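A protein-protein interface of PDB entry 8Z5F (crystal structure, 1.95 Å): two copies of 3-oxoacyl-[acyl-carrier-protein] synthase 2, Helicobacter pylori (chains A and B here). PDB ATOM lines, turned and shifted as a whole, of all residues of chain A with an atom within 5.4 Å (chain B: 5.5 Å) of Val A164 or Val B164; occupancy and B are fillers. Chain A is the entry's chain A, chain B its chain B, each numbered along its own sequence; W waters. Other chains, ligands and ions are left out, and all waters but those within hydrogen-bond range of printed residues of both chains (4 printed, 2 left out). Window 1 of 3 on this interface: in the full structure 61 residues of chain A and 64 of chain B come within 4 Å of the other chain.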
ATOM      1  N   SER A 110      19.325  23.287   1.300  1.00  0.00           N
ATOM      2  CA  SER A 110      19.431  22.214   0.316  1.00  0.00           C
ATOM      3  C   SER A 110      18.441  22.472  -0.812  1.00  0.00           C
ATOM      4  O   SER A 110      17.371  23.060  -0.597  1.00  0.00           O
ATOM      5  CB  SER A 110      19.169  20.829   0.927  1.00  0.00           C
ATOM      6  OG  SER A 110      19.591  19.812   0.030  1.00  0.00           O
ATOM      7  N   GLY A 111      18.763  21.965  -2.006  1.00  0.00           N
ATOM      8  CA  GLY A 111      17.876  22.148  -3.173  1.00  0.00           C
ATOM      9  C   GLY A 111      16.692  21.194  -3.170  1.00  0.00           C
ATOM     10  O   GLY A 111      15.569  21.664  -3.430  1.00  0.00           O
ATOM     11  N   ILE A 112      16.924  19.902  -2.906  1.00  0.00           N
ATOM     12  CA  ILE A 112      15.816  18.899  -2.981  1.00  0.00           C
ATOM     13  C   ILE A 112      15.918  17.916  -1.807  1.00  0.00           C
ATOM     14  O   ILE A 112      14.913  17.239  -1.524  1.00  0.00           O
ATOM     15  CB  ILE A 112      15.833  18.162  -4.335  1.00  0.00           C
ATOM     16  CG1 ILE A 112      14.486  17.500  -4.640  1.00  0.00           C
ATOM     17  CG2 ILE A 112      16.979  17.165  -4.393  1.00  0.00           C
ATOM     18  CD1 ILE A 112      14.402  16.888  -6.017  1.00  0.00           C
ATOM     19  N   VAL A 143      14.088  18.479   3.279  1.00  0.00           N
ATOM     20  CA  VAL A 143      15.224  19.401   3.372  1.00  0.00           C
ATOM     21  C   VAL A 143      15.450  19.865   4.807  1.00  0.00           C
ATOM     22  O   VAL A 143      16.595  19.963   5.276  1.00  0.00           O
ATOM     23  CB  VAL A 143      15.017  20.611   2.437  1.00  0.00           C
ATOM     24  CG1 VAL A 143      16.120  21.662   2.660  1.00  0.00           C
ATOM     25  CG2 VAL A 143      14.947  20.160   0.956  1.00  0.00           C
ATOM     26  N   ASN A 144      14.373  20.167   5.533  1.00  0.00           N
ATOM     27  CA  ASN A 144      14.565  20.777   6.841  1.00  0.00           C
ATOM     28  C   ASN A 144      14.996  19.772   7.890  1.00  0.00           C
ATOM     29  O   ASN A 144      15.377  20.178   8.996  1.00  0.00           O
ATOM     30  CB  ASN A 144      13.302  21.501   7.302  1.00  0.00           C
ATOM     31  CG  ASN A 144      12.182  20.542   7.683  1.00  0.00           C
ATOM     32  OD1 ASN A 144      11.766  19.713   6.886  1.00  0.00           O
ATOM     33  ND2 ASN A 144      11.709  20.644   8.911  1.00  0.00           N
ATOM     34  N   SER A 162      15.179  26.852   7.210  1.00  0.00           N
ATOM     35  CA  SER A 162      15.704  26.073   6.097  1.00  0.00           C
ATOM     36  C   SER A 162      15.383  26.756   4.775  1.00  0.00           C
ATOM     37  O   SER A 162      14.225  27.099   4.521  1.00  0.00           O
ATOM     38  CB  SER A 162      15.132  24.647   6.126  1.00  0.00           C
ATOM     39  OG  SER A 162      16.066  23.713   5.612  1.00  0.00           O
ATOM     40  N   SER A 163      16.411  26.935   3.938  1.00  0.00           N
ATOM     41  CA  SER A 163      16.298  27.586   2.641  1.00  0.00           C
ATOM     42  C   SER A 163      16.376  26.529   1.540  1.00  0.00           C
ATOM     43  O   SER A 163      17.148  25.570   1.637  1.00  0.00           O
ATOM     44  CB  SER A 163      17.403  28.641   2.443  1.00  0.00           C
ATOM     45  OG  SER A 163      17.471  29.582   3.519  1.00  0.00           O
ATOM     46  N   VAL A 164      15.576  26.704   0.494  1.00  0.00           N
ATOM     47  CA  VAL A 164      15.464  25.688  -0.543  1.00  0.00           C
ATOM     48  C   VAL A 164      15.575  26.369  -1.915  1.00  0.00           C
ATOM     49  O   VAL A 164      15.000  25.914  -2.909  1.00  0.00           O
ATOM     50  CB  VAL A 164      14.150  24.890  -0.348  1.00  0.00           C
ATOM     51  CG1 VAL A 164      12.926  25.760  -0.576  1.00  0.00           C
ATOM     52  CG2 VAL A 164      14.098  23.635  -1.214  1.00  0.00           C
ATOM     53  N   THR A 165      16.340  27.464  -1.977  1.00  0.00           N
ATOM     54  CA  THR A 165      16.507  28.204  -3.229  1.00  0.00           C
ATOM     55  C   THR A 165      17.517  27.570  -4.176  1.00  0.00           C
ATOM     56  O   THR A 165      18.444  28.251  -4.635  1.00  0.00           O
ATOM     57  CB  THR A 165      16.898  29.655  -2.956  1.00  0.00           C
ATOM     58  OG1 THR A 165      17.693  29.719  -1.768  1.00  0.00           O
ATOM     59  CG2 THR A 165      15.641  30.583  -2.864  1.00  0.00           C
ATOM     60  N   ALA A 166      17.321  26.287  -4.506  1.00  0.00           N
ATOM     61  CA  ALA A 166      18.039  25.660  -5.607  1.00  0.00           C
ATOM     62  C   ALA A 166      19.565  25.769  -5.431  1.00  0.00           C
ATOM     63  O   ALA A 166      20.056  25.512  -4.343  1.00  0.00           O
ATOM     64  CB  ALA A 166      17.588  26.282  -6.933  1.00  0.00           C
ATOM     65  N   ALA A 169      20.820  27.867  -2.420  1.00  0.00           N
ATOM     66  CA  ALA A 169      20.350  27.539  -1.071  1.00  0.00           C
ATOM     67  C   ALA A 169      21.449  27.665  -0.021  1.00  0.00           C
ATOM     68  O   ALA A 169      21.200  28.177   1.076  1.00  0.00           O
ATOM     69  CB  ALA A 169      19.770  26.123  -1.042  1.00  0.00           C
ATOM     70  N   SER B 110       6.886  25.829   0.974  1.00  0.00           N
ATOM     71  CA  SER B 110       6.278  24.517   0.788  1.00  0.00           C
ATOM     72  C   SER B 110       7.099  23.505   1.574  1.00  0.00           C
ATOM     73  O   SER B 110       8.304  23.693   1.801  1.00  0.00           O
ATOM     74  CB  SER B 110       6.204  24.123  -0.692  1.00  0.00           C
ATOM     75  OG  SER B 110       5.495  22.903  -0.884  1.00  0.00           O
ATOM     76  N   GLY B 111       6.468  22.368   1.873  1.00  0.00           N
ATOM     77  CA  GLY B 111       7.151  21.262   2.571  1.00  0.00           C
ATOM     78  C   GLY B 111       7.953  20.371   1.636  1.00  0.00           C
ATOM     79  O   GLY B 111       9.114  20.101   1.949  1.00  0.00           O
ATOM     80  N   ILE B 112       7.338  19.921   0.536  1.00  0.00           N
ATOM     81  CA  ILE B 112       8.033  18.997  -0.409  1.00  0.00           C
ATOM     82  C   ILE B 112       7.919  19.503  -1.857  1.00  0.00           C
ATOM     83  O   ILE B 112       8.688  19.019  -2.689  1.00  0.00           O
ATOM     84  CB  ILE B 112       7.520  17.549  -0.267  1.00  0.00           C
ATOM     85  CG1 ILE B 112       8.554  16.534  -0.761  1.00  0.00           C
ATOM     86  CG2 ILE B 112       6.180  17.384  -0.966  1.00  0.00           C
ATOM     87  CD1 ILE B 112       8.439  15.174  -0.119  1.00  0.00           C
ATOM     88  N   VAL B 143      10.811  23.431  -4.728  1.00  0.00           N
ATOM     89  CA  VAL B 143       9.942  24.271  -3.902  1.00  0.00           C
ATOM     90  C   VAL B 143      10.083  25.746  -4.274  1.00  0.00           C
ATOM     91  O   VAL B 143       9.087  26.481  -4.311  1.00  0.00           O
ATOM     92  CB  VAL B 143      10.234  24.027  -2.408  1.00  0.00           C
ATOM     93  CG1 VAL B 143       9.564  25.117  -1.511  1.00  0.00           C
ATOM     94  CG2 VAL B 143       9.788  22.610  -2.017  1.00  0.00           C
ATOM     95  N   ASN B 144      11.317  26.207  -4.562  1.00  0.00           N
ATOM     96  CA  ASN B 144      11.527  27.637  -4.821  1.00  0.00           C
ATOM     97  C   ASN B 144      11.011  28.064  -6.183  1.00  0.00           C
ATOM     98  O   ASN B 144      10.960  29.265  -6.467  1.00  0.00           O
ATOM     99  CB  ASN B 144      13.005  28.006  -4.719  1.00  0.00           C
ATOM    100  CG  ASN B 144      13.797  27.484  -5.880  1.00  0.00           C
ATOM    101  OD1 ASN B 144      13.910  26.265  -6.055  1.00  0.00           O
ATOM    102  ND2 ASN B 144      14.333  28.389  -6.705  1.00  0.00           N
ATOM    103  N   SER B 162      12.864  31.163  -0.130  1.00  0.00           N
ATOM    104  CA  SER B 162      11.988  30.011  -0.049  1.00  0.00           C
ATOM    105  C   SER B 162      12.261  29.252   1.241  1.00  0.00           C
ATOM    106  O   SER B 162      13.407  28.880   1.527  1.00  0.00           O
ATOM    107  CB  SER B 162      12.179  29.117  -1.272  1.00  0.00           C
ATOM    108  OG  SER B 162      10.981  28.423  -1.603  1.00  0.00           O
ATOM    109  N   SER B 163      11.197  29.035   2.014  1.00  0.00           N
ATOM    110  CA  SER B 163      11.249  28.282   3.263  1.00  0.00           C
ATOM    111  C   SER B 163      10.710  26.865   3.063  1.00  0.00           C
ATOM    112  O   SER B 163       9.688  26.664   2.400  1.00  0.00           O
ATOM    113  CB  SER B 163      10.441  29.001   4.346  1.00  0.00           C
ATOM    114  OG  SER B 163      10.842  30.362   4.492  1.00  0.00           O
ATOM    115  N   VAL B 164      11.374  25.882   3.668  1.00  0.00           N
ATOM    116  CA  VAL B 164      10.980  24.488   3.476  1.00  0.00           C
ATOM    117  C   VAL B 164      10.912  23.789   4.832  1.00  0.00           C
ATOM    118  O   VAL B 164      11.269  22.613   4.958  1.00  0.00           O
ATOM    119  CB  VAL B 164      11.943  23.795   2.489  1.00  0.00           C
ATOM    120  CG1 VAL B 164      13.357  23.731   3.051  1.00  0.00           C
ATOM    121  CG2 VAL B 164      11.434  22.419   2.028  1.00  0.00           C
ATOM    122  N   THR B 165      10.434  24.503   5.859  1.00  0.00           N
ATOM    123  CA  THR B 165      10.365  23.935   7.208  1.00  0.00           C
ATOM    124  C   THR B 165       9.054  23.169   7.423  1.00  0.00           C
ATOM    125  O   THR B 165       8.261  23.476   8.313  1.00  0.00           O
ATOM    126  CB  THR B 165      10.544  25.015   8.275  1.00  0.00           C
ATOM    127  OG1 THR B 165       9.940  26.245   7.858  1.00  0.00           O
ATOM    128  CG2 THR B 165      12.036  25.219   8.592  1.00  0.00           C
ATOM    129  N   ALA B 166       8.863  22.139   6.597  1.00  0.00           N
ATOM    130  CA  ALA B 166       7.798  21.162   6.767  1.00  0.00           C
ATOM    131  C   ALA B 166       6.451  21.852   6.987  1.00  0.00           C
ATOM    132  O   ALA B 166       6.121  22.779   6.247  1.00  0.00           O
ATOM    133  CB  ALA B 166       8.140  20.212   7.907  1.00  0.00           C
ATOM    134  N   ALA B 169       6.263  25.774   7.114  1.00  0.00           N
ATOM    135  CA  ALA B 169       6.855  26.560   6.034  1.00  0.00           C
ATOM    136  C   ALA B 169       6.036  27.807   5.708  1.00  0.00           C
ATOM    137  O   ALA B 169       6.603  28.885   5.480  1.00  0.00           O
ATOM    138  CB  ALA B 169       7.019  25.684   4.784  1.00  0.00           C
HETATM  139  O   HOH W   1      12.456  21.304  -3.774  1.00  0.00           O
HETATM  140  O   HOH W   2      11.764  19.136   1.349  1.00  0.00           O
HETATM  141  O   HOH W   3      15.864  29.882   0.284  1.00  0.00           O
HETATM  142  O   HOH W   4      14.309  30.248   4.235  1.00  0.00           O
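The backbone carbonyl oxygen (O) of Val A164 lies close to the side-chain amide oxygen (OD1) of Asn B144 (3.3 Å).
O of Ser A162 sits at hydrogen-bond distance from N of Val B164, 3.2 Å away.
N of Val A164 sits at hydrogen-bond distance from O of Ser B162, 3.2 Å away.
The backbone NH of Ser B110 lies within hydrogen-bond range of the backbone carbonyl oxygen of Ser B163.
The backbone NH (N) of Ser A110 is in hydrogen-bond range of the backbone carbonyl oxygen (O) of Ser A163, at 3.2 Å.
Val A143 touches Val B164.
Asn A144 touches Val B164.
Asn A144 touches Ala B166 (ND2 to CB, 3.7 Å).
O of Ser A162 touches O of Ser B162, 3.6 Å away.
Ser A162 touches Ser B163 (O to CA, 3.4 Å).
O of Ser B162 touches CA of Ser A163, at 3.4 Å.
Val B164 touches Val A164.
CB of Asn B144 touches CA of Thr A165, at 3.8 Å.
Thr A165 touches Ser B162.
Asn B144 touches Ala A166.
Printed residues of chain B within 4 Å of Asn A144: Val B164 (3.3 Å), Thr B165 (3.8 Å) and Ala B166 (3.7 Å).
Of chain B, only Val B143, Asn B144, Ser B162 and Val B164 come within 4 Å of Val A164.
Of the printed residues of chain B, Thr A165 touches Asn B144 and Ser B162.
Printed residues of chain B within 4 Å of Ala A166: Asn B144.
Ser B110 touches none of the printed residues of chain A.
Of the printed residues of chain A, Val B143 touches Val A164.
Printed residues of chain A within 4 Å of Ser B162: Ser A162 (3.6 Å), Ser A163 (3.4 Å), Val A164 (3.2 Å) and Thr A165 (3.9 Å).
The nearest residue of chain B that does not touch Val A164 is Ser B163 (4.4 Å).
The nearest residue of chain A that does not touch Val B164 is Ser A163 (4.4 Å).
The nearest printed residue of chain B that does not touch Asn A144 is Gly B111 (5.6 Å).
Of the 11 printed residues of chain B, 7 touch a printed residue of chain A.
Along chain B the printed residues that touch a printed residue of chain A span positions 143 to 166.
Val A143 touches Val B164, and with the chains exchanged Val A164 touches Val B143.
Ser A162 touches Ser B163, and with the chains exchanged Ser A163 touches Ser B162.
Ser A162 touches Val B164, and with the chains exchanged Val A164 touches Ser B162.
Val B164 touches its own counterpart, Val A164.
Water W3 lies within hydrogen-bond range of OG1 of Thr A165 (2.8 Å), O of Ser B162 (2.9 Å) and N of Val A164 (3.2 Å).
Water W1 lies within hydrogen-bond range of the backbone NH of Val B143 (2.9 Å) and the backbone carbonyl oxygen of Gly A111 (3.2 Å).
Water W2 bridges the backbone carbonyl oxygen of Gly B111 (2.9 Å) and the backbone NH of Val A143 (3.1 Å).
Water W4 lies within hydrogen-bond range of O of Ser A162 (3.2 Å), O of Ser B162 (3.2 Å), OG of Ser A163 (3.3 Å) and OG of Ser B163 (3.5 Å).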
